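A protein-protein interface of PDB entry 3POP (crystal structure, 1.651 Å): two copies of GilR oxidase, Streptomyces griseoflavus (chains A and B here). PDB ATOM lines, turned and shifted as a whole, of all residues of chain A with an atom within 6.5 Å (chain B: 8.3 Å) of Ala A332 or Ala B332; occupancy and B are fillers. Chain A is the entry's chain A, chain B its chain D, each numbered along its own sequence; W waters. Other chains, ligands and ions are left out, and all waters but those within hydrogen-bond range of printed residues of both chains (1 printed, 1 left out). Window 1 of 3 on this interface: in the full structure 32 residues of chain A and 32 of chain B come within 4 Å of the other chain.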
ATOM      1  N   ALA A 127      31.013 -31.936  -1.227  1.00  0.00           N
ATOM      2  CA  ALA A 127      30.384 -30.953  -2.078  1.00  0.00           C
ATOM      3  C   ALA A 127      29.108 -30.352  -1.490  1.00  0.00           C
ATOM      4  O   ALA A 127      28.454 -29.551  -2.148  1.00  0.00           O
ATOM      5  CB  ALA A 127      30.076 -31.587  -3.418  1.00  0.00           C
ATOM      6  N   CYS A 128      28.731 -30.747  -0.279  1.00  0.00           N
ATOM      7  CA  CYS A 128      27.521 -30.195   0.350  1.00  0.00           C
ATOM      8  C   CYS A 128      27.921 -29.398   1.570  1.00  0.00           C
ATOM      9  O   CYS A 128      28.430 -29.969   2.541  1.00  0.00           O
ATOM     10  CB  CYS A 128      26.580 -31.331   0.795  1.00  0.00           C
ATOM     11  SG  CYS A 128      26.114 -32.530  -0.507  1.00  0.00           S
ATOM     12  N   SER A 129      27.693 -28.084   1.540  1.00  0.00           N
ATOM     13  CA  SER A 129      28.297 -27.236   2.544  1.00  0.00           C
ATOM     14  C   SER A 129      27.603 -27.277   3.916  1.00  0.00           C
ATOM     15  O   SER A 129      28.156 -26.797   4.903  1.00  0.00           O
ATOM     16  CB  SER A 129      28.408 -25.800   2.020  1.00  0.00           C
ATOM     17  OG  SER A 129      27.138 -25.306   1.686  1.00  0.00           O
ATOM     18  N   ALA A 130      26.415 -27.872   3.997  1.00  0.00           N
ATOM     19  CA  ALA A 130      25.733 -27.977   5.285  1.00  0.00           C
ATOM     20  C   ALA A 130      26.069 -29.240   6.097  1.00  0.00           C
ATOM     21  O   ALA A 130      25.650 -29.379   7.248  1.00  0.00           O
ATOM     22  CB  ALA A 130      24.207 -27.886   5.070  1.00  0.00           C
ATOM     23  N   SER A 330      29.101 -26.234  -5.527  1.00  0.00           N
ATOM     24  CA  SER A 330      28.583 -26.873  -4.297  1.00  0.00           C
ATOM     25  C   SER A 330      27.091 -26.727  -4.083  1.00  0.00           C
ATOM     26  O   SER A 330      26.444 -25.910  -4.721  1.00  0.00           O
ATOM     27  CB  SER A 330      29.274 -26.313  -3.049  1.00  0.00           C
ATOM     28  OG  SER A 330      30.644 -26.689  -2.985  1.00  0.00           O
ATOM     29  N   GLN A 331      26.566 -27.503  -3.133  1.00  0.00           N
ATOM     30  CA  GLN A 331      25.140 -27.478  -2.776  1.00  0.00           C
ATOM     31  C   GLN A 331      24.999 -26.946  -1.352  1.00  0.00           C
ATOM     32  O   GLN A 331      25.542 -27.527  -0.424  1.00  0.00           O
ATOM     33  CB  GLN A 331      24.557 -28.899  -2.876  1.00  0.00           C
ATOM     34  CG  GLN A 331      23.112 -29.057  -2.381  1.00  0.00           C
ATOM     35  CD  GLN A 331      22.150 -28.159  -3.129  1.00  0.00           C
ATOM     36  OE1 GLN A 331      21.893 -28.359  -4.315  1.00  0.00           O
ATOM     37  NE2 GLN A 331      21.625 -27.149  -2.443  1.00  0.00           N
ATOM     38  N   ALA A 332      24.289 -25.836  -1.162  1.00  0.00           N
ATOM     39  CA  ALA A 332      24.101 -25.323   0.195  1.00  0.00           C
ATOM     40  C   ALA A 332      22.740 -25.691   0.789  1.00  0.00           C
ATOM     41  O   ALA A 332      21.912 -26.322   0.129  1.00  0.00           O
ATOM     42  CB  ALA A 332      24.328 -23.797   0.240  1.00  0.00           C
ATOM     43  N   ASP A 333      22.520 -25.328   2.050  1.00  0.00           N
ATOM     44  CA  ASP A 333      21.225 -25.574   2.694  1.00  0.00           C
ATOM     45  C   ASP A 333      20.185 -24.506   2.324  1.00  0.00           C
ATOM     46  O   ASP A 333      19.827 -23.658   3.141  1.00  0.00           O
ATOM     47  CB  ASP A 333      21.364 -25.711   4.228  1.00  0.00           C
ATOM     48  CG  ASP A 333      22.056 -24.512   4.881  1.00  0.00           C
ATOM     49  OD1 ASP A 333      22.924 -23.885   4.226  1.00  0.00           O
ATOM     50  OD2 ASP A 333      21.743 -24.214   6.065  1.00  0.00           O
ATOM     51  N   CYS A 334      19.707 -24.562   1.084  1.00  0.00           N
ATOM     52  CA  CYS A 334      18.703 -23.622   0.607  1.00  0.00           C
ATOM     53  C   CYS A 334      17.900 -24.216  -0.544  1.00  0.00           C
ATOM     54  O   CYS A 334      18.325 -25.175  -1.193  1.00  0.00           O
ATOM     55  CB  CYS A 334      19.357 -22.318   0.138  1.00  0.00           C
ATOM     56  SG  CYS A 334      20.435 -22.539  -1.335  1.00  0.00           S
ATOM     57  N   GLY A 335      16.728 -23.636  -0.800  1.00  0.00           N
ATOM     58  CA  GLY A 335      15.930 -24.061  -1.939  1.00  0.00           C
ATOM     59  C   GLY A 335      15.364 -25.472  -1.824  1.00  0.00           C
ATOM     60  O   GLY A 335      15.088 -25.962  -0.722  1.00  0.00           O
ATOM     61  N   VAL A 337      16.247 -28.516  -1.939  1.00  0.00           N
ATOM     62  CA  VAL A 337      16.820 -29.649  -1.198  1.00  0.00           C
ATOM     63  C   VAL A 337      16.358 -29.651   0.263  1.00  0.00           C
ATOM     64  O   VAL A 337      16.553 -30.632   0.983  1.00  0.00           O
ATOM     65  CB  VAL A 337      18.367 -29.671  -1.246  1.00  0.00           C
ATOM     66  CG1 VAL A 337      18.854 -29.763  -2.696  1.00  0.00           C
ATOM     67  CG2 VAL A 337      18.954 -28.435  -0.520  1.00  0.00           C
ATOM     68  N   MET A 338      15.738 -28.549   0.696  1.00  0.00           N
ATOM     69  CA  MET A 338      15.322 -28.379   2.094  1.00  0.00           C
ATOM     70  C   MET A 338      13.932 -28.951   2.361  1.00  0.00           C
ATOM     71  O   MET A 338      13.026 -28.814   1.543  1.00  0.00           O
ATOM     72  CB  MET A 338      15.350 -26.897   2.492  1.00  0.00           C
ATOM     73  CG  MET A 338      16.716 -26.240   2.309  1.00  0.00           C
ATOM     74  SD  MET A 338      17.999 -27.100   3.300  1.00  0.00           S
ATOM     75  CE  MET A 338      17.380 -26.867   4.974  1.00  0.00           C
ATOM     76  N   ASP B  27      30.266 -10.117  -4.430  1.00  0.00           N
ATOM     77  CA  ASP B  27      29.329 -10.999  -5.106  1.00  0.00           C
ATOM     78  C   ASP B  27      29.122 -10.687  -6.599  1.00  0.00           C
ATOM     79  O   ASP B  27      29.036 -11.600  -7.427  1.00  0.00           O
ATOM     80  CB  ASP B  27      27.988 -11.023  -4.397  1.00  0.00           C
ATOM     81  CG  ASP B  27      27.166 -12.253  -4.791  1.00  0.00           C
ATOM     82  OD1 ASP B  27      27.604 -13.407  -4.517  1.00  0.00           O
ATOM     83  OD2 ASP B  27      26.095 -12.054  -5.398  1.00  0.00           O
ATOM     84  N   HIS B  68      27.469  -7.872  -0.944  1.00  0.00           N
ATOM     85  CA  HIS B  68      26.319  -7.907  -1.859  1.00  0.00           C
ATOM     86  C   HIS B  68      25.968  -6.629  -2.611  1.00  0.00           C
ATOM     87  O   HIS B  68      24.970  -6.587  -3.316  1.00  0.00           O
ATOM     88  CB  HIS B  68      25.093  -8.518  -1.171  1.00  0.00           C
ATOM     89  CG  HIS B  68      24.991  -9.980  -1.433  1.00  0.00           C
ATOM     90  ND1 HIS B  68      24.247 -10.486  -2.477  1.00  0.00           N
ATOM     91  CD2 HIS B  68      25.656 -11.030  -0.891  1.00  0.00           C
ATOM     92  CE1 HIS B  68      24.433 -11.793  -2.548  1.00  0.00           C
ATOM     93  NE2 HIS B  68      25.282 -12.150  -1.593  1.00  0.00           N
ATOM     94  N   ASP B 109      22.162 -15.437   7.170  1.00  0.00           N
ATOM     95  CA  ASP B 109      22.075 -16.832   7.602  1.00  0.00           C
ATOM     96  C   ASP B 109      22.497 -17.001   9.050  1.00  0.00           C
ATOM     97  O   ASP B 109      21.826 -17.680   9.840  1.00  0.00           O
ATOM     98  CB  ASP B 109      22.986 -17.705   6.745  1.00  0.00           C
ATOM     99  CG  ASP B 109      22.706 -19.188   6.946  1.00  0.00           C
ATOM    100  OD1 ASP B 109      23.675 -19.948   7.165  1.00  0.00           O
ATOM    101  OD2 ASP B 109      21.517 -19.589   6.880  1.00  0.00           O
ATOM    102  N   LYS B 113      19.800 -18.112  12.085  1.00  0.00           N
ATOM    103  CA  LYS B 113      20.040 -19.317  12.880  1.00  0.00           C
ATOM    104  C   LYS B 113      20.223 -18.989  14.357  1.00  0.00           C
ATOM    105  O   LYS B 113      19.665 -19.676  15.222  1.00  0.00           O
ATOM    106  CB  LYS B 113      21.244 -20.095  12.344  1.00  0.00           C
ATOM    107  CG  LYS B 113      20.902 -20.846  11.066  1.00  0.00           C
ATOM    108  CD  LYS B 113      22.128 -21.351  10.312  1.00  0.00           C
ATOM    109  CE  LYS B 113      21.688 -22.160   9.091  1.00  0.00           C
ATOM    110  NZ  LYS B 113      22.820 -22.418   8.140  1.00  0.00           N
ATOM    111  N   ALA B 127      15.692 -12.272   1.868  1.00  0.00           N
ATOM    112  CA  ALA B 127      15.566 -13.638   1.348  1.00  0.00           C
ATOM    113  C   ALA B 127      16.898 -14.218   0.830  1.00  0.00           C
ATOM    114  O   ALA B 127      16.944 -15.331   0.293  1.00  0.00           O
ATOM    115  CB  ALA B 127      14.522 -13.644   0.226  1.00  0.00           C
ATOM    116  N   CYS B 128      17.991 -13.474   0.985  1.00  0.00           N
ATOM    117  CA  CYS B 128      19.295 -13.946   0.528  1.00  0.00           C
ATOM    118  C   CYS B 128      20.180 -14.128   1.746  1.00  0.00           C
ATOM    119  O   CYS B 128      20.534 -13.154   2.414  1.00  0.00           O
ATOM    120  CB  CYS B 128      19.932 -12.926  -0.422  1.00  0.00           C
ATOM    121  SG  CYS B 128      18.934 -12.469  -1.896  1.00  0.00           S
ATOM    122  N   SER B 129      20.561 -15.360   2.037  1.00  0.00           N
ATOM    123  CA  SER B 129      21.181 -15.618   3.328  1.00  0.00           C
ATOM    124  C   SER B 129      22.651 -15.189   3.418  1.00  0.00           C
ATOM    125  O   SER B 129      23.203 -15.109   4.516  1.00  0.00           O
ATOM    126  CB  SER B 129      21.002 -17.081   3.721  1.00  0.00           C
ATOM    127  OG  SER B 129      21.578 -17.906   2.747  1.00  0.00           O
ATOM    128  N   ALA B 130      23.272 -14.865   2.287  1.00  0.00           N
ATOM    129  CA  ALA B 130      24.669 -14.426   2.294  1.00  0.00           C
ATOM    130  C   ALA B 130      24.882 -12.912   2.460  1.00  0.00           C
ATOM    131  O   ALA B 130      26.009 -12.432   2.608  1.00  0.00           O
ATOM    132  CB  ALA B 130      25.355 -14.907   1.025  1.00  0.00           C
ATOM    133  N   VAL B 131      23.803 -12.154   2.428  1.00  0.00           N
ATOM    134  CA  VAL B 131      23.881 -10.699   2.608  1.00  0.00           C
ATOM    135  C   VAL B 131      24.451 -10.343   3.984  1.00  0.00           C
ATOM    136  O   VAL B 131      24.130 -10.979   4.982  1.00  0.00           O
ATOM    137  CB  VAL B 131      22.474 -10.076   2.432  1.00  0.00           C
ATOM    138  CG1 VAL B 131      22.435  -8.627   2.939  1.00  0.00           C
ATOM    139  CG2 VAL B 131      22.031 -10.177   0.962  1.00  0.00           C
ATOM    140  N   ARG B 327      14.625 -21.450   4.943  1.00  0.00           N
ATOM    141  CA  ARG B 327      15.660 -21.838   3.991  1.00  0.00           C
ATOM    142  C   ARG B 327      15.100 -22.367   2.683  1.00  0.00           C
ATOM    143  O   ARG B 327      15.661 -22.125   1.617  1.00  0.00           O
ATOM    144  CB  ARG B 327      16.614 -22.858   4.637  1.00  0.00           C
ATOM    145  CG  ARG B 327      17.519 -22.151   5.640  1.00  0.00           C
ATOM    146  CD  ARG B 327      18.401 -23.132   6.377  1.00  0.00           C
ATOM    147  NE  ARG B 327      17.606 -24.061   7.173  1.00  0.00           N
ATOM    148  CZ  ARG B 327      18.108 -25.089   7.850  1.00  0.00           C
ATOM    149  NH1 ARG B 327      17.304 -25.888   8.551  1.00  0.00           N
ATOM    150  NH2 ARG B 327      19.415 -25.320   7.819  1.00  0.00           N
ATOM    151  N   MET B 329      12.575 -21.254   1.209  1.00  0.00           N
ATOM    152  CA  MET B 329      12.157 -20.099   0.422  1.00  0.00           C
ATOM    153  C   MET B 329      13.313 -19.139   0.087  1.00  0.00           C
ATOM    154  O   MET B 329      13.090 -18.124  -0.571  1.00  0.00           O
ATOM    155  CB  MET B 329      11.058 -19.321   1.164  1.00  0.00           C
ATOM    156  CG  MET B 329       9.817 -20.158   1.501  1.00  0.00           C
ATOM    157  SD  MET B 329       9.002 -20.771   0.002  1.00  0.00           S
ATOM    158  CE  MET B 329       7.953 -19.340  -0.339  1.00  0.00           C
ATOM    159  N   SER B 330      14.530 -19.448   0.545  1.00  0.00           N
ATOM    160  CA  SER B 330      15.664 -18.501   0.446  1.00  0.00           C
ATOM    161  C   SER B 330      16.711 -18.861  -0.601  1.00  0.00           C
ATOM    162  O   SER B 330      16.741 -19.972  -1.118  1.00  0.00           O
ATOM    163  CB  SER B 330      16.397 -18.378   1.785  1.00  0.00           C
ATOM    164  OG  SER B 330      15.580 -17.750   2.763  1.00  0.00           O
ATOM    165  N   GLN B 331      17.592 -17.903  -0.879  1.00  0.00           N
ATOM    166  CA  GLN B 331      18.698 -18.080  -1.823  1.00  0.00           C
ATOM    167  C   GLN B 331      20.017 -18.044  -1.042  1.00  0.00           C
ATOM    168  O   GLN B 331      20.314 -17.049  -0.391  1.00  0.00           O
ATOM    169  CB  GLN B 331      18.663 -16.959  -2.870  1.00  0.00           C
ATOM    170  CG  GLN B 331      19.857 -16.932  -3.834  1.00  0.00           C
ATOM    171  CD  GLN B 331      19.998 -18.228  -4.608  1.00  0.00           C
ATOM    172  OE1 GLN B 331      19.169 -18.545  -5.461  1.00  0.00           O
ATOM    173  NE2 GLN B 331      21.036 -18.996  -4.299  1.00  0.00           N
ATOM    174  N   ALA B 332      20.804 -19.123  -1.081  1.00  0.00           N
ATOM    175  CA  ALA B 332      22.103 -19.107  -0.389  1.00  0.00           C
ATOM    176  C   ALA B 332      23.279 -18.808  -1.332  1.00  0.00           C
ATOM    177  O   ALA B 332      23.091 -18.655  -2.545  1.00  0.00           O
ATOM    178  CB  ALA B 332      22.340 -20.412   0.383  1.00  0.00           C
ATOM    179  N   ASP B 333      24.485 -18.707  -0.769  1.00  0.00           N
ATOM    180  CA  ASP B 333      25.698 -18.514  -1.582  1.00  0.00           C
ATOM    181  C   ASP B 333      26.218 -19.827  -2.198  1.00  0.00           C
ATOM    182  O   ASP B 333      27.259 -20.371  -1.786  1.00  0.00           O
ATOM    183  CB  ASP B 333      26.806 -17.774  -0.804  1.00  0.00           C
ATOM    184  CG  ASP B 333      27.180 -18.455   0.517  1.00  0.00           C
ATOM    185  OD1 ASP B 333      26.318 -19.110   1.137  1.00  0.00           O
ATOM    186  OD2 ASP B 333      28.350 -18.317   0.948  1.00  0.00           O
ATOM    187  N   CYS B 334      25.478 -20.343  -3.176  1.00  0.00           N
ATOM    188  CA  CYS B 334      25.879 -21.573  -3.853  1.00  0.00           C
ATOM    189  C   CYS B 334      25.319 -21.645  -5.265  1.00  0.00           C
ATOM    190  O   CYS B 334      24.367 -20.941  -5.607  1.00  0.00           O
ATOM    191  CB  CYS B 334      25.418 -22.802  -3.058  1.00  0.00           C
ATOM    192  SG  CYS B 334      23.605 -22.907  -2.945  1.00  0.00           S
ATOM    193  N   GLY B 335      25.925 -22.492  -6.095  1.00  0.00           N
ATOM    194  CA  GLY B 335      25.394 -22.732  -7.424  1.00  0.00           C
ATOM    195  C   GLY B 335      25.488 -21.539  -8.361  1.00  0.00           C
ATOM    196  O   GLY B 335      26.417 -20.724  -8.256  1.00  0.00           O
ATOM    197  N   ASP B 336      24.519 -21.427  -9.266  1.00  0.00           N
ATOM    198  CA  ASP B 336      24.631 -20.514 -10.404  1.00  0.00           C
ATOM    199  C   ASP B 336      24.617 -19.019 -10.082  1.00  0.00           C
ATOM    200  O   ASP B 336      24.958 -18.197 -10.944  1.00  0.00           O
ATOM    201  CB  ASP B 336      23.572 -20.839 -11.462  1.00  0.00           C
ATOM    202  CG  ASP B 336      23.836 -22.162 -12.149  1.00  0.00           C
ATOM    203  OD1 ASP B 336      25.025 -22.482 -12.384  1.00  0.00           O
ATOM    204  OD2 ASP B 336      22.857 -22.887 -12.438  1.00  0.00           O
ATOM    205  N   VAL B 337      24.242 -18.656  -8.862  1.00  0.00           N
ATOM    206  CA  VAL B 337      24.280 -17.235  -8.488  1.00  0.00           C
ATOM    207  C   VAL B 337      25.705 -16.785  -8.167  1.00  0.00           C
ATOM    208  O   VAL B 337      25.960 -15.586  -8.032  1.00  0.00           O
ATOM    209  CB  VAL B 337      23.345 -16.903  -7.293  1.00  0.00           C
ATOM    210  CG1 VAL B 337      21.905 -17.282  -7.638  1.00  0.00           C
ATOM    211  CG2 VAL B 337      23.821 -17.607  -6.006  1.00  0.00           C
ATOM    212  N   MET B 338      26.634 -17.747  -8.053  1.00  0.00           N
ATOM    213  CA  MET B 338      28.020 -17.442  -7.669  1.00  0.00           C
ATOM    214  C   MET B 338      28.924 -17.109  -8.858  1.00  0.00           C
ATOM    215  O   MET B 338      28.861 -17.751  -9.917  1.00  0.00           O
ATOM    216  CB  MET B 338      28.641 -18.602  -6.876  1.00  0.00           C
ATOM    217  CG  MET B 338      27.862 -18.982  -5.624  1.00  0.00           C
ATOM    218  SD  MET B 338      27.714 -17.618  -4.442  1.00  0.00           S
ATOM    219  CE  MET B 338      29.443 -17.262  -4.107  1.00  0.00           C
HETATM  220  O   HOH W   1      18.490 -21.377  -3.546  1.00  0.00           O
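Among the printed residues, merely in contact across the chains: Met A338 with Arg B327 (3.5 Å), Cys A334 with Arg B327 (3.5 Å), Ser A330 with Cys B334 (3.7 Å), Gly A335 with Ser B330 (3.7 Å), Ser A330 with Gly B335 (3.7 Å), Cys A334 with Ser B330 (3.7 Å) and Ala A332 with Ala B332 (3.9 Å).
Of the 12 printed residues of chain A, 6 touch a printed residue of chain B.
Hydrophobic or aromatic side chains of chain A within 4 Å of the printed part of chain B: Ala A332 and Met A338.
Hydrophobic or aromatic side chains of chain B within 4 Å of the printed part of chain A: Ala B332.
Among the printed residues, 13 pairs touch across the chains.
Among the printed residues, Asp or Glu carboxylates within 4 Å of a Lys or Arg side-chain nitrogen of the other chain: Asp A333 with Lys B113 (2.9 Å) and Asp A333 with Arg B327 (3.1 Å).
Ser A330 touches Cys B334, and with the chains exchanged Cys A334 touches Ser B330.
Ser A330 touches Gly B335, and with the chains exchanged Gly A335 touches Ser B330.
Ala B332 touches its own counterpart, Ala A332.
Ala A332 touches Cys B334, and with the chains exchanged Cys A334 touches Ala B332.
Positions printed for both chains: 127, 128, 129, 130, 330, 331, 332, 333, 334, 335, 337 and 338.
Of the 13 pairs that touch across the chains among the printed residues, 8 have their exchanged pair printed and touching as well.
Water W1 lies within hydrogen-bond range of SG of Cys A334 (3.2 Å), O of Ser B330 (3.3 Å) and OE1 of Gln B331 (3.5 Å).
SD of Met B338 lies close to N of Cys B334, 3.7 Å away.
N of Cys A334 sits close to SD of Met A338 (3.8 Å).
The side-chain amino group of Lys B113 lies within salt-bridge range of the side-chain carboxylate of Asp B109 (2.8 Å).
OD2 of Asp A333 lies within salt-bridge range of NH2 of Arg B327.
The side-chain carboxylate of Asp A333 lies within salt-bridge range of the side-chain amino group of Lys B113 (2.9 Å).
The backbone NH (N) of Gly A335 sits at hydrogen-bond distance from the backbone carbonyl oxygen (O) of Arg B327 (3.0 Å).
SG of Cys B334 lies close to N of Ala A332, at 3.5 Å.
The side-chain sulfur (SG) of Cys A334 sits at hydrogen-bond distance from the side-chain sulfur (SG) of Cys B334, at 3.6 Å.
The side-chain sulfur (SG) of Cys A334 sits close to the backbone NH (N) of Ala B332 (3.4 Å).
Of the printed residues of chain B, Cys A334 touches Arg B327 (3.5 Å), Ser B330 (3.7 Å), Ala B332 (3.3 Å) and Cys B334 (3.6 Å).
Of the printed residues of chain A, Lys B113 touches Asp A333.
Printed residues of chain A within 4 Å of Cys B334: Ser A330, Ala A332 and Cys A334.
Of the printed residues of chain A, Gly B335 touches Ser A330.
Asp B336 touches none of the printed residues of chain A.
The nearest residue of chain B that does not touch Ala A332 is Asp B333 (4.9 Å).
The nearest printed residue of chain B that does not touch Cys A334 is Gln B331 (4.5 Å).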
